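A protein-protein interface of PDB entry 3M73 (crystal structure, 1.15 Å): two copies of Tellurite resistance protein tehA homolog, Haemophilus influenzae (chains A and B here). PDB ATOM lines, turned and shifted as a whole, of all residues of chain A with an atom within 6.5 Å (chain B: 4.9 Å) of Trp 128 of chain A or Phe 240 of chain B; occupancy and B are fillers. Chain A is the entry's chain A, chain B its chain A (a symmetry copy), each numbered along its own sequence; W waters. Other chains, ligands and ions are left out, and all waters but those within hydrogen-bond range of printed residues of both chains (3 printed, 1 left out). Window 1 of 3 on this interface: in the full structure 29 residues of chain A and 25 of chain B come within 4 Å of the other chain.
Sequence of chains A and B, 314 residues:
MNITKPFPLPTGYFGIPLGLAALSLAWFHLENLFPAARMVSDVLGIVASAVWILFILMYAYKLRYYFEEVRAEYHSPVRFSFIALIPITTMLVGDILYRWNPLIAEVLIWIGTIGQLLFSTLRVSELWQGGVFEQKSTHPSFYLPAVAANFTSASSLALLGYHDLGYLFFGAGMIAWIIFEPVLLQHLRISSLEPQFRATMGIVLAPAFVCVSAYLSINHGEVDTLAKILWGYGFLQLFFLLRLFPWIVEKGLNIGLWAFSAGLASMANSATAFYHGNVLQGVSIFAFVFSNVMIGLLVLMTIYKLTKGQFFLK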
ATOM      1  N   LEU A 117      -7.512  14.690   7.271  1.00  0.00           N
ATOM      2  CA  LEU A 117      -8.007  15.833   6.542  1.00  0.00           C
ATOM      3  C   LEU A 117      -7.853  17.097   7.389  1.00  0.00           C
ATOM      4  O   LEU A 117      -7.467  18.161   6.888  1.00  0.00           O
ATOM      5  CB  LEU A 117      -9.460  15.614   6.150  1.00  0.00           C
ATOM      6  CG  LEU A 117     -10.103  16.726   5.348  1.00  0.00           C
ATOM      7  CD1 LEU A 117      -9.373  17.002   4.051  1.00  0.00           C
ATOM      8  CD2 LEU A 117     -11.560  16.389   5.079  1.00  0.00           C
ATOM      9  N   SER A 120      -3.994  18.034   7.326  1.00  0.00           N
ATOM     10  CA  SER A 120      -3.554  18.707   6.108  1.00  0.00           C
ATOM     11  C   SER A 120      -4.168  20.090   5.982  1.00  0.00           C
ATOM     12  O   SER A 120      -3.497  21.048   5.591  1.00  0.00           O
ATOM     13  CB  SER A 120      -3.884  17.892   4.870  1.00  0.00           C
ATOM     14  OG  SER A 120      -5.277  17.780   4.675  1.00  0.00           O
ATOM     15  N   THR A 121      -5.451  20.192   6.278  1.00  0.00           N
ATOM     16  CA  THR A 121      -6.128  21.467   6.200  1.00  0.00           C
ATOM     17  C   THR A 121      -5.450  22.486   7.091  1.00  0.00           C
ATOM     18  O   THR A 121      -5.319  23.659   6.723  1.00  0.00           O
ATOM     19  CB  THR A 121      -7.604  21.309   6.570  1.00  0.00           C
ATOM     20  OG1 THR A 121      -8.233  20.520   5.561  1.00  0.00           O
ATOM     21  CG2 THR A 121      -8.310  22.640   6.644  1.00  0.00           C
ATOM     22  N   LEU A 122      -4.999  22.083   8.261  1.00  0.00           N
ATOM     23  CA  LEU A 122      -4.295  22.994   9.162  1.00  0.00           C
ATOM     24  C   LEU A 122      -2.876  23.284   8.722  1.00  0.00           C
ATOM     25  O   LEU A 122      -2.458  24.436   8.745  1.00  0.00           O
ATOM     26  CB  LEU A 122      -4.260  22.433  10.575  1.00  0.00           C
ATOM     27  CG  LEU A 122      -5.615  22.416  11.272  1.00  0.00           C
ATOM     28  CD1 LEU A 122      -5.561  21.656  12.578  1.00  0.00           C
ATOM     29  CD2 LEU A 122      -6.095  23.825  11.489  1.00  0.00           C
ATOM     30  N   ARG A 123      -2.110  22.256   8.357  1.00  0.00           N
ATOM     31  CA  ARG A 123      -0.675  22.418   8.145  1.00  0.00           C
ATOM     32  C   ARG A 123      -0.196  22.512   6.729  1.00  0.00           C
ATOM     33  O   ARG A 123       0.704  23.305   6.455  1.00  0.00           O
ATOM     34  CB  ARG A 123       0.081  21.301   8.830  1.00  0.00           C
ATOM     35  CG  ARG A 123       0.006  21.474  10.277  1.00  0.00           C
ATOM     36  CD  ARG A 123       0.810  22.699  10.710  1.00  0.00           C
ATOM     37  NE  ARG A 123       2.221  22.457  10.460  1.00  0.00           N
ATOM     38  CZ  ARG A 123       3.034  23.186   9.702  1.00  0.00           C
ATOM     39  NH1 ARG A 123       2.632  24.331   9.161  1.00  0.00           N
ATOM     40  NH2 ARG A 123       4.277  22.789   9.531  1.00  0.00           N
ATOM     41  N   VAL A 124      -0.734  21.713   5.815  1.00  0.00           N
ATOM     42  CA  VAL A 124      -0.287  21.769   4.424  1.00  0.00           C
ATOM     43  C   VAL A 124      -0.627  23.124   3.819  1.00  0.00           C
ATOM     44  O   VAL A 124       0.196  23.743   3.137  1.00  0.00           O
ATOM     45  CB  VAL A 124      -0.849  20.608   3.601  1.00  0.00           C
ATOM     46  CG1 VAL A 124      -0.492  20.760   2.106  1.00  0.00           C
ATOM     47  CG2 VAL A 124      -0.286  19.308   4.106  1.00  0.00           C
ATOM     48  N   SER A 125      -1.853  23.603   4.091  1.00  0.00           N
ATOM     49  CA  SER A 125      -2.267  24.901   3.587  1.00  0.00           C
ATOM     50  C   SER A 125      -1.428  26.036   4.187  1.00  0.00           C
ATOM     51  O   SER A 125      -1.134  27.016   3.531  1.00  0.00           O
ATOM     52  CB  SER A 125      -3.737  25.148   3.888  1.00  0.00           C
ATOM     53  OG  SER A 125      -3.907  25.308   5.273  1.00  0.00           O
ATOM     54  N   GLU A 126      -1.086  25.920   5.478  1.00  0.00           N
ATOM     55  CA  GLU A 126      -0.344  26.968   6.158  1.00  0.00           C
ATOM     56  C   GLU A 126       0.986  27.250   5.467  1.00  0.00           C
ATOM     57  O   GLU A 126       1.489  28.395   5.530  1.00  0.00           O
ATOM     58  CB  GLU A 126      -0.095  26.555   7.617  1.00  0.00           C
ATOM     59  CG  GLU A 126       0.470  27.627   8.460  1.00  0.00           C
ATOM     60  CD  GLU A 126       0.571  27.229   9.916  1.00  0.00           C
ATOM     61  OE1 GLU A 126       0.585  26.017  10.272  1.00  0.00           O
ATOM     62  OE2 GLU A 126       0.717  28.167  10.748  1.00  0.00           O
ATOM     63  N   LEU A 127       1.569  26.243   4.856  1.00  0.00           N
ATOM     64  CA  LEU A 127       2.810  26.443   4.151  1.00  0.00           C
ATOM     65  C   LEU A 127       2.698  27.528   3.066  1.00  0.00           C
ATOM     66  O   LEU A 127       3.671  28.221   2.788  1.00  0.00           O
ATOM     67  CB  LEU A 127       3.282  25.129   3.541  1.00  0.00           C
ATOM     68  CG  LEU A 127       3.529  23.967   4.488  1.00  0.00           C
ATOM     69  CD1 LEU A 127       3.851  22.710   3.699  1.00  0.00           C
ATOM     70  CD2 LEU A 127       4.645  24.261   5.465  1.00  0.00           C
ATOM     71  N   TRP A 128       1.500  27.667   2.487  1.00  0.00           N
ATOM     72  CA  TRP A 128       1.280  28.630   1.412  1.00  0.00           C
ATOM     73  C   TRP A 128       1.368  30.078   1.877  1.00  0.00           C
ATOM     74  O   TRP A 128       1.342  30.986   1.055  1.00  0.00           O
ATOM     75  CB  TRP A 128      -0.072  28.435   0.728  1.00  0.00           C
ATOM     76  CG  TRP A 128      -0.348  27.143   0.040  1.00  0.00           C
ATOM     77  CD1 TRP A 128       0.470  26.035  -0.111  1.00  0.00           C
ATOM     78  CD2 TRP A 128      -1.553  26.811  -0.606  1.00  0.00           C
ATOM     79  NE1 TRP A 128      -0.178  25.043  -0.801  1.00  0.00           N
ATOM     80  CE2 TRP A 128      -1.429  25.502  -1.118  1.00  0.00           C
ATOM     81  CE3 TRP A 128      -2.768  27.472  -0.747  1.00  0.00           C
ATOM     82  CZ2 TRP A 128      -2.463  24.874  -1.768  1.00  0.00           C
ATOM     83  CZ3 TRP A 128      -3.781  26.844  -1.415  1.00  0.00           C
ATOM     84  CH2 TRP A 128      -3.630  25.548  -1.903  1.00  0.00           C
ATOM     85  N   GLN A 129       1.497  30.326   3.192  1.00  0.00           N
ATOM     86  CA  GLN A 129       1.750  31.660   3.714  1.00  0.00           C
ATOM     87  C   GLN A 129       3.179  32.136   3.492  1.00  0.00           C
ATOM     88  O   GLN A 129       3.464  33.317   3.645  1.00  0.00           O
ATOM     89  CB  GLN A 129       1.451  31.728   5.210  1.00  0.00           C
ATOM     90  CG  GLN A 129      -0.003  31.450   5.537  1.00  0.00           C
ATOM     91  CD  GLN A 129      -0.267  31.414   7.017  1.00  0.00           C
ATOM     92  OE1 GLN A 129       0.664  31.513   7.823  1.00  0.00           O
ATOM     93  NE2 GLN A 129      -1.514  31.266   7.394  1.00  0.00           N
ATOM     94  N   GLY A 130       4.073  31.230   3.139  1.00  0.00           N
ATOM     95  CA  GLY A 130       5.434  31.561   2.798  1.00  0.00           C
ATOM     96  C   GLY A 130       6.341  31.799   3.978  1.00  0.00           C
ATOM     97  O   GLY A 130       5.916  32.046   5.089  1.00  0.00           O
ATOM     98  N   PHE A 142       6.879  14.817   2.299  1.00  0.00           N
ATOM     99  CA  PHE A 142       5.674  15.605   2.030  1.00  0.00           C
ATOM    100  C   PHE A 142       4.565  14.759   1.417  1.00  0.00           C
ATOM    101  O   PHE A 142       3.386  15.045   1.590  1.00  0.00           O
ATOM    102  CB  PHE A 142       6.044  16.810   1.156  1.00  0.00           C
ATOM    103  CG  PHE A 142       4.919  17.748   0.855  1.00  0.00           C
ATOM    104  CD1 PHE A 142       4.659  18.838   1.649  1.00  0.00           C
ATOM    105  CD2 PHE A 142       4.134  17.547  -0.283  1.00  0.00           C
ATOM    106  CE1 PHE A 142       3.632  19.720   1.286  1.00  0.00           C
ATOM    107  CE2 PHE A 142       3.115  18.393  -0.620  1.00  0.00           C
ATOM    108  CZ  PHE A 142       2.866  19.489   0.177  1.00  0.00           C
ATOM    109  N   LEU B 185       2.451  26.459  -6.448  1.00  0.00           N
ATOM    110  CA  LEU B 185       2.342  26.122  -5.020  1.00  0.00           C
ATOM    111  C   LEU B 185       3.712  26.095  -4.359  1.00  0.00           C
ATOM    112  O   LEU B 185       3.842  26.472  -3.203  1.00  0.00           O
ATOM    113  CB  LEU B 185       1.589  24.821  -4.804  1.00  0.00           C
ATOM    114  CG  LEU B 185       0.149  24.780  -5.359  1.00  0.00           C
ATOM    115  CD1 LEU B 185      -0.541  23.505  -4.897  1.00  0.00           C
ATOM    116  CD2 LEU B 185      -0.652  26.016  -4.997  1.00  0.00           C
ATOM    117  N   LEU B 188       4.415  29.703  -3.600  1.00  0.00           N
ATOM    118  CA  LEU B 188       3.644  30.170  -2.450  1.00  0.00           C
ATOM    119  C   LEU B 188       4.245  29.648  -1.142  1.00  0.00           C
ATOM    120  O   LEU B 188       4.326  30.355  -0.147  1.00  0.00           O
ATOM    121  CB  LEU B 188       2.182  29.777  -2.545  1.00  0.00           C
ATOM    122  CG  LEU B 188       1.419  30.359  -3.719  1.00  0.00           C
ATOM    123  CD1 LEU B 188      -0.024  29.844  -3.700  1.00  0.00           C
ATOM    124  CD2 LEU B 188       1.451  31.859  -3.647  1.00  0.00           C
ATOM    125  N   ARG B 189       4.715  28.396  -1.140  1.00  0.00           N
ATOM    126  CA  ARG B 189       5.323  27.841   0.061  1.00  0.00           C
ATOM    127  C   ARG B 189       6.560  28.624   0.460  1.00  0.00           C
ATOM    128  O   ARG B 189       6.797  28.844   1.649  1.00  0.00           O
ATOM    129  CB  ARG B 189       5.718  26.377  -0.148  1.00  0.00           C
ATOM    130  CG  ARG B 189       4.568  25.383  -0.082  1.00  0.00           C
ATOM    131  CD  ARG B 189       5.058  23.936  -0.007  1.00  0.00           C
ATOM    132  NE  ARG B 189       5.530  23.445  -1.303  1.00  0.00           N
ATOM    133  CZ  ARG B 189       4.757  22.867  -2.213  1.00  0.00           C
ATOM    134  NH1 ARG B 189       3.468  22.676  -1.976  1.00  0.00           N
ATOM    135  NH2 ARG B 189       5.277  22.466  -3.368  1.00  0.00           N
ATOM    136  N   SER B 192       5.330  33.080  -0.984  1.00  0.00           N
ATOM    137  CA  SER B 192       3.960  33.550  -0.895  1.00  0.00           C
ATOM    138  C   SER B 192       3.724  34.799  -1.715  1.00  0.00           C
ATOM    139  O   SER B 192       4.484  35.066  -2.667  1.00  0.00           O
ATOM    140  CB  SER B 192       3.537  33.756   0.563  1.00  0.00           C
ATOM    141  OG  SER B 192       2.103  33.802   0.656  1.00  0.00           O
ATOM    142  N   MET B 201      -5.295  34.862  -4.218  1.00  0.00           N
ATOM    143  CA  MET B 201      -5.307  33.500  -3.719  1.00  0.00           C
ATOM    144  C   MET B 201      -6.642  32.833  -4.053  1.00  0.00           C
ATOM    145  O   MET B 201      -6.700  31.616  -4.219  1.00  0.00           O
ATOM    146  CB  MET B 201      -5.071  33.481  -2.207  1.00  0.00           C
ATOM    147  CG  MET B 201      -3.621  33.694  -1.803  1.00  0.00           C
ATOM    148  SD  MET B 201      -2.504  32.497  -2.556  1.00  0.00           S
ATOM    149  CE  MET B 201      -2.945  31.011  -1.657  1.00  0.00           C
ATOM    150  N   VAL B 204      -6.889  30.348  -6.878  1.00  0.00           N
ATOM    151  CA  VAL B 204      -6.463  28.974  -6.655  1.00  0.00           C
ATOM    152  C   VAL B 204      -7.663  28.033  -6.481  1.00  0.00           C
ATOM    153  O   VAL B 204      -7.547  26.843  -6.731  1.00  0.00           O
ATOM    154  CB  VAL B 204      -5.464  28.888  -5.467  1.00  0.00           C
ATOM    155  CG1 VAL B 204      -5.043  27.459  -5.147  1.00  0.00           C
ATOM    156  CG2 VAL B 204      -4.240  29.773  -5.716  1.00  0.00           C
ATOM    157  N   LEU B 236     -10.471  19.789  -1.617  1.00  0.00           N
ATOM    158  CA  LEU B 236      -9.234  19.927  -0.866  1.00  0.00           C
ATOM    159  C   LEU B 236      -8.789  21.388  -0.879  1.00  0.00           C
ATOM    160  O   LEU B 236      -8.469  21.985   0.168  1.00  0.00           O
ATOM    161  CB  LEU B 236      -8.150  19.037  -1.467  1.00  0.00           C
ATOM    162  CG  LEU B 236      -6.833  19.022  -0.702  1.00  0.00           C
ATOM    163  CD1 LEU B 236      -6.934  18.176   0.520  1.00  0.00           C
ATOM    164  CD2 LEU B 236      -5.702  18.575  -1.621  1.00  0.00           C
ATOM    165  N   GLN B 237      -8.740  21.988  -2.064  1.00  0.00           N
ATOM    166  CA  GLN B 237      -8.289  23.375  -2.180  1.00  0.00           C
ATOM    167  C   GLN B 237      -9.237  24.332  -1.460  1.00  0.00           C
ATOM    168  O   GLN B 237      -8.773  25.303  -0.859  1.00  0.00           O
ATOM    169  CB  GLN B 237      -8.160  23.773  -3.645  1.00  0.00           C
ATOM    170  CG  GLN B 237      -7.175  22.928  -4.486  1.00  0.00           C
ATOM    171  CD  GLN B 237      -5.753  23.054  -4.034  1.00  0.00           C
ATOM    172  OE1 GLN B 237      -5.387  22.605  -2.943  1.00  0.00           O
ATOM    173  NE2 GLN B 237      -4.926  23.703  -4.850  1.00  0.00           N
ATOM    174  N   LEU B 238     -10.528  24.064  -1.535  1.00  0.00           N
ATOM    175  CA  LEU B 238     -11.495  24.856  -0.786  1.00  0.00           C
ATOM    176  C   LEU B 238     -11.178  24.834   0.715  1.00  0.00           C
ATOM    177  O   LEU B 238     -11.155  25.892   1.357  1.00  0.00           O
ATOM    178  CB  LEU B 238     -12.905  24.363  -1.010  1.00  0.00           C
ATOM    179  CG  LEU B 238     -13.995  25.078  -0.181  1.00  0.00           C
ATOM    180  CD1 LEU B 238     -14.096  26.541  -0.533  1.00  0.00           C
ATOM    181  CD2 LEU B 238     -15.327  24.368  -0.338  1.00  0.00           C
ATOM    182  N   PHE B 239     -10.963  23.644   1.278  1.00  0.00           N
ATOM    183  CA  PHE B 239     -10.625  23.546   2.686  1.00  0.00           C
ATOM    184  C   PHE B 239      -9.374  24.311   3.009  1.00  0.00           C
ATOM    185  O   PHE B 239      -9.307  25.008   4.026  1.00  0.00           O
ATOM    186  CB  PHE B 239     -10.505  22.096   3.120  1.00  0.00           C
ATOM    187  CG  PHE B 239     -11.790  21.322   3.020  1.00  0.00           C
ATOM    188  CD1 PHE B 239     -13.021  21.934   2.880  1.00  0.00           C
ATOM    189  CD2 PHE B 239     -11.746  19.995   2.747  1.00  0.00           C
ATOM    190  CE1 PHE B 239     -14.175  21.185   2.729  1.00  0.00           C
ATOM    191  CE2 PHE B 239     -12.889  19.250   2.604  1.00  0.00           C
ATOM    192  CZ  PHE B 239     -14.095  19.860   2.594  1.00  0.00           C
ATOM    193  N   PHE B 240      -8.356  24.182   2.173  1.00  0.00           N
ATOM    194  CA  PHE B 240      -7.106  24.892   2.388  1.00  0.00           C
ATOM    195  C   PHE B 240      -7.333  26.401   2.394  1.00  0.00           C
ATOM    196  O   PHE B 240      -6.821  27.120   3.257  1.00  0.00           O
ATOM    197  CB  PHE B 240      -6.082  24.517   1.314  1.00  0.00           C
ATOM    198  CG  PHE B 240      -5.469  23.130   1.466  1.00  0.00           C
ATOM    199  CD1 PHE B 240      -5.880  22.191   2.402  1.00  0.00           C
ATOM    200  CD2 PHE B 240      -4.470  22.746   0.598  1.00  0.00           C
ATOM    201  CE1 PHE B 240      -5.271  20.958   2.492  1.00  0.00           C
ATOM    202  CE2 PHE B 240      -3.877  21.471   0.688  1.00  0.00           C
ATOM    203  CZ  PHE B 240      -4.278  20.607   1.621  1.00  0.00           C
ATOM    204  N   LEU B 241      -8.095  26.881   1.432  1.00  0.00           N
ATOM    205  CA  LEU B 241      -8.317  28.303   1.305  1.00  0.00           C
ATOM    206  C   LEU B 241      -9.209  28.841   2.431  1.00  0.00           C
ATOM    207  O   LEU B 241      -9.022  29.979   2.869  1.00  0.00           O
ATOM    208  CB  LEU B 241      -8.882  28.645  -0.074  1.00  0.00           C
ATOM    209  CG  LEU B 241      -7.853  28.481  -1.200  1.00  0.00           C
ATOM    210  CD1 LEU B 241      -8.548  28.459  -2.544  1.00  0.00           C
ATOM    211  CD2 LEU B 241      -6.800  29.582  -1.167  1.00  0.00           C
ATOM    212  N   LEU B 242     -10.150  28.038   2.915  1.00  0.00           N
ATOM    213  CA  LEU B 242     -10.929  28.432   4.070  1.00  0.00           C
ATOM    214  C   LEU B 242     -10.024  28.626   5.277  1.00  0.00           C
ATOM    215  O   LEU B 242     -10.132  29.612   6.011  1.00  0.00           O
ATOM    216  CB  LEU B 242     -11.984  27.380   4.347  1.00  0.00           C
ATOM    217  CG  LEU B 242     -13.223  27.414   3.448  1.00  0.00           C
ATOM    218  CD1 LEU B 242     -14.061  26.175   3.663  1.00  0.00           C
ATOM    219  CD2 LEU B 242     -14.050  28.642   3.726  1.00  0.00           C
ATOM    220  N   ARG B 243      -9.105  27.686   5.505  1.00  0.00           N
ATOM    221  CA  ARG B 243      -8.175  27.811   6.605  1.00  0.00           C
ATOM    222  C   ARG B 243      -7.306  29.059   6.458  1.00  0.00           C
ATOM    223  O   ARG B 243      -7.004  29.732   7.444  1.00  0.00           O
ATOM    224  CB  ARG B 243      -7.334  26.545   6.717  1.00  0.00           C
ATOM    225  CG  ARG B 243      -6.435  26.482   7.927  1.00  0.00           C
ATOM    226  CD  ARG B 243      -5.083  27.093   7.671  1.00  0.00           C
ATOM    227  NE  ARG B 243      -4.083  26.737   8.677  1.00  0.00           N
ATOM    228  CZ  ARG B 243      -3.918  27.355   9.813  1.00  0.00           C
ATOM    229  NH1 ARG B 243      -4.670  28.414  10.099  1.00  0.00           N
ATOM    230  NH2 ARG B 243      -2.995  26.925  10.662  1.00  0.00           N
ATOM    231  N   LEU B 244      -6.916  29.364   5.234  1.00  0.00           N
ATOM    232  CA  LEU B 244      -6.055  30.505   4.932  1.00  0.00           C
ATOM    233  C   LEU B 244      -6.812  31.830   4.911  1.00  0.00           C
ATOM    234  O   LEU B 244      -6.170  32.877   4.827  1.00  0.00           O
ATOM    235  CB  LEU B 244      -5.384  30.293   3.582  1.00  0.00           C
ATOM    236  CG  LEU B 244      -4.262  29.257   3.582  1.00  0.00           C
ATOM    237  CD1 LEU B 244      -3.882  28.877   2.211  1.00  0.00           C
ATOM    238  CD2 LEU B 244      -3.044  29.765   4.367  1.00  0.00           C
ATOM    239  N   TRP B 247      -5.696  34.941   6.964  1.00  0.00           N
ATOM    240  CA  TRP B 247      -4.444  35.433   6.420  1.00  0.00           C
ATOM    241  C   TRP B 247      -4.648  36.173   5.107  1.00  0.00           C
ATOM    242  O   TRP B 247      -4.054  37.241   4.855  1.00  0.00           O
ATOM    243  CB  TRP B 247      -3.421  34.303   6.286  1.00  0.00           C
ATOM    244  CG  TRP B 247      -2.153  34.596   5.512  1.00  0.00           C
ATOM    245  CD1 TRP B 247      -0.979  35.158   5.998  1.00  0.00           C
ATOM    246  CD2 TRP B 247      -1.899  34.289   4.142  1.00  0.00           C
ATOM    247  NE1 TRP B 247      -0.052  35.209   5.002  1.00  0.00           N
ATOM    248  CE2 TRP B 247      -0.588  34.718   3.844  1.00  0.00           C
ATOM    249  CE3 TRP B 247      -2.651  33.693   3.134  1.00  0.00           C
ATOM    250  CZ2 TRP B 247      -0.029  34.566   2.584  1.00  0.00           C
ATOM    251  CZ3 TRP B 247      -2.102  33.562   1.893  1.00  0.00           C
ATOM    252  CH2 TRP B 247      -0.811  33.977   1.619  1.00  0.00           C
HETATM  253  O   HOH W   1       0.221  21.855  -1.454  1.00  0.00           O
HETATM  254  O   HOH W   2       2.784  35.658   5.163  1.00  0.00           O
HETATM  255  O   HOH W   3       1.770  22.959   0.573  1.00  0.00           O
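The guanidinium group of Arg 243 of chain B is in hydrogen-bond range of the backbone carbonyl oxygen of Leu 122 of chain A (2.8 Å).
OE1 of Glu 126 of chain A lies within salt-bridge range of NH2 of Arg 243 of chain B (3.7 Å).
O of Trp 128 of chain A sits at hydrogen-bond distance from OG of Ser 192 of chain B, at 2.9 Å.
The backbone carbonyl oxygen (O) of Gln 129 of chain A sits close to the side-chain hydroxyl (OG) of Ser 192 of chain B (3.3 Å).
N of Gly 130 of chain A lies close to O of Leu 188 of chain B (3.4 Å).
The backbone carbonyl oxygen of Leu 127 of chain A lies close to the backbone carbonyl oxygen of Arg 189 of chain B.
The backbone carbonyl oxygen of Leu 188 of chain B lies close to the backbone carbonyl oxygen of Trp 128 of chain A, at 3.3 Å.
The side-chain hydroxyl (OG) of Ser 120 of chain A is in hydrogen-bond range of the backbone carbonyl oxygen (O) of Leu 117 of chain A.
O of Leu 117 of chain A lies within hydrogen-bond range of OG1 of Thr 121 of chain A, 2.8 Å away.
The backbone NH (N) of Ser 125 of chain A sits at hydrogen-bond distance from the backbone carbonyl oxygen (O) of Ser 120 of chain A.
The side-chain hydroxyl of Ser 125 of chain A is in hydrogen-bond range of the backbone carbonyl oxygen of Thr 121 of chain A (2.6 Å).
NH1 of Arg 123 of chain A is in salt-bridge range of OE1 of Glu 126 of chain A.
CG2 of Thr 121 of chain A touches O of Phe 239 of chain B, 3.7 Å away.
CE2 of Phe 240 of chain B touches CG1 of Val 124 of chain A, at 3.7 Å.
Ser 125 of chain A touches Leu 244 of chain B (O to CD2, 3.5 Å).
Trp 128 of chain A touches Leu 185 of chain B.
Val 204 of chain B touches Trp 128 of chain A (CG1 to CZ3, 3.99 Å).
Phe 240 of chain B touches Trp 128 of chain A (CD2 to CZ2, 3.8 Å).
CH2 of Trp 247 of chain B touches O of Trp 128 of chain A, 3.7 Å away.
Gln 129 of chain A touches Leu 244 of chain B (CG to CD2, 3.7 Å).
Gln 129 of chain A touches Trp 247 of chain B.
Gly 130 of chain A touches Ser 192 of chain B.
Printed residues of chain B within 4 Å of Thr 121 of chain A: Phe 239 (3.7 Å), Phe 240 (3.8 Å) and Arg 243 (3.3 Å).
Of the printed residues of chain B, Leu 122 of chain A touches Arg 243 (2.8 Å).
Of the printed residues of chain B, Trp 128 of chain A touches Leu 185, Leu 188, Ser 192, Met 201, Val 204, Gln 237, Phe 240, Leu 244 and Trp 247.
Of the printed residues of chain A, Ser 192 of chain B touches Trp 128, Gln 129 and Gly 130.
Printed residues of chain A within 4 Å of Gln 237 of chain B: Trp 128.
The nearest printed residue of chain B that does not touch Trp 128 of chain A is Leu 241 of chain B (4.1 Å).
Hydrophobic or aromatic side chains of chain B that line the printed part of chain A: Leu 185, Leu 188, Met 201, Val 204, Phe 239, Phe 240, Leu 244 and Trp 247.
Hydrophobic or aromatic side chains of chain A within 4 Å of the printed part of chain B: Val 124, Leu 127, Trp 128 and Phe 142.
Among the printed residues, Asp or Glu carboxylates within 4 Å of a Lys or Arg side-chain nitrogen of the other chain: Glu 126 of chain A with Arg 243 of chain B (3.7 Å).
No position is printed for both chains.
Water W2 lies within hydrogen-bond range of O of Gln 129 of chain A (2.9 Å) and NE1 of Trp 247 of chain B (2.9 Å).
Water W3 lies within hydrogen-bond range of the guanidinium group of Arg 189 of chain B (3.1 Å), the backbone carbonyl oxygen of Val 124 of chain A (3.1 Å) and the indole nitrogen of Trp 128 of chain A (3.2 Å).
Water W1 lies within hydrogen-bond range of NE1 of Trp 128 of chain A (3.3 Å) and NH1 of Arg 189 of chain B (3.4 Å).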
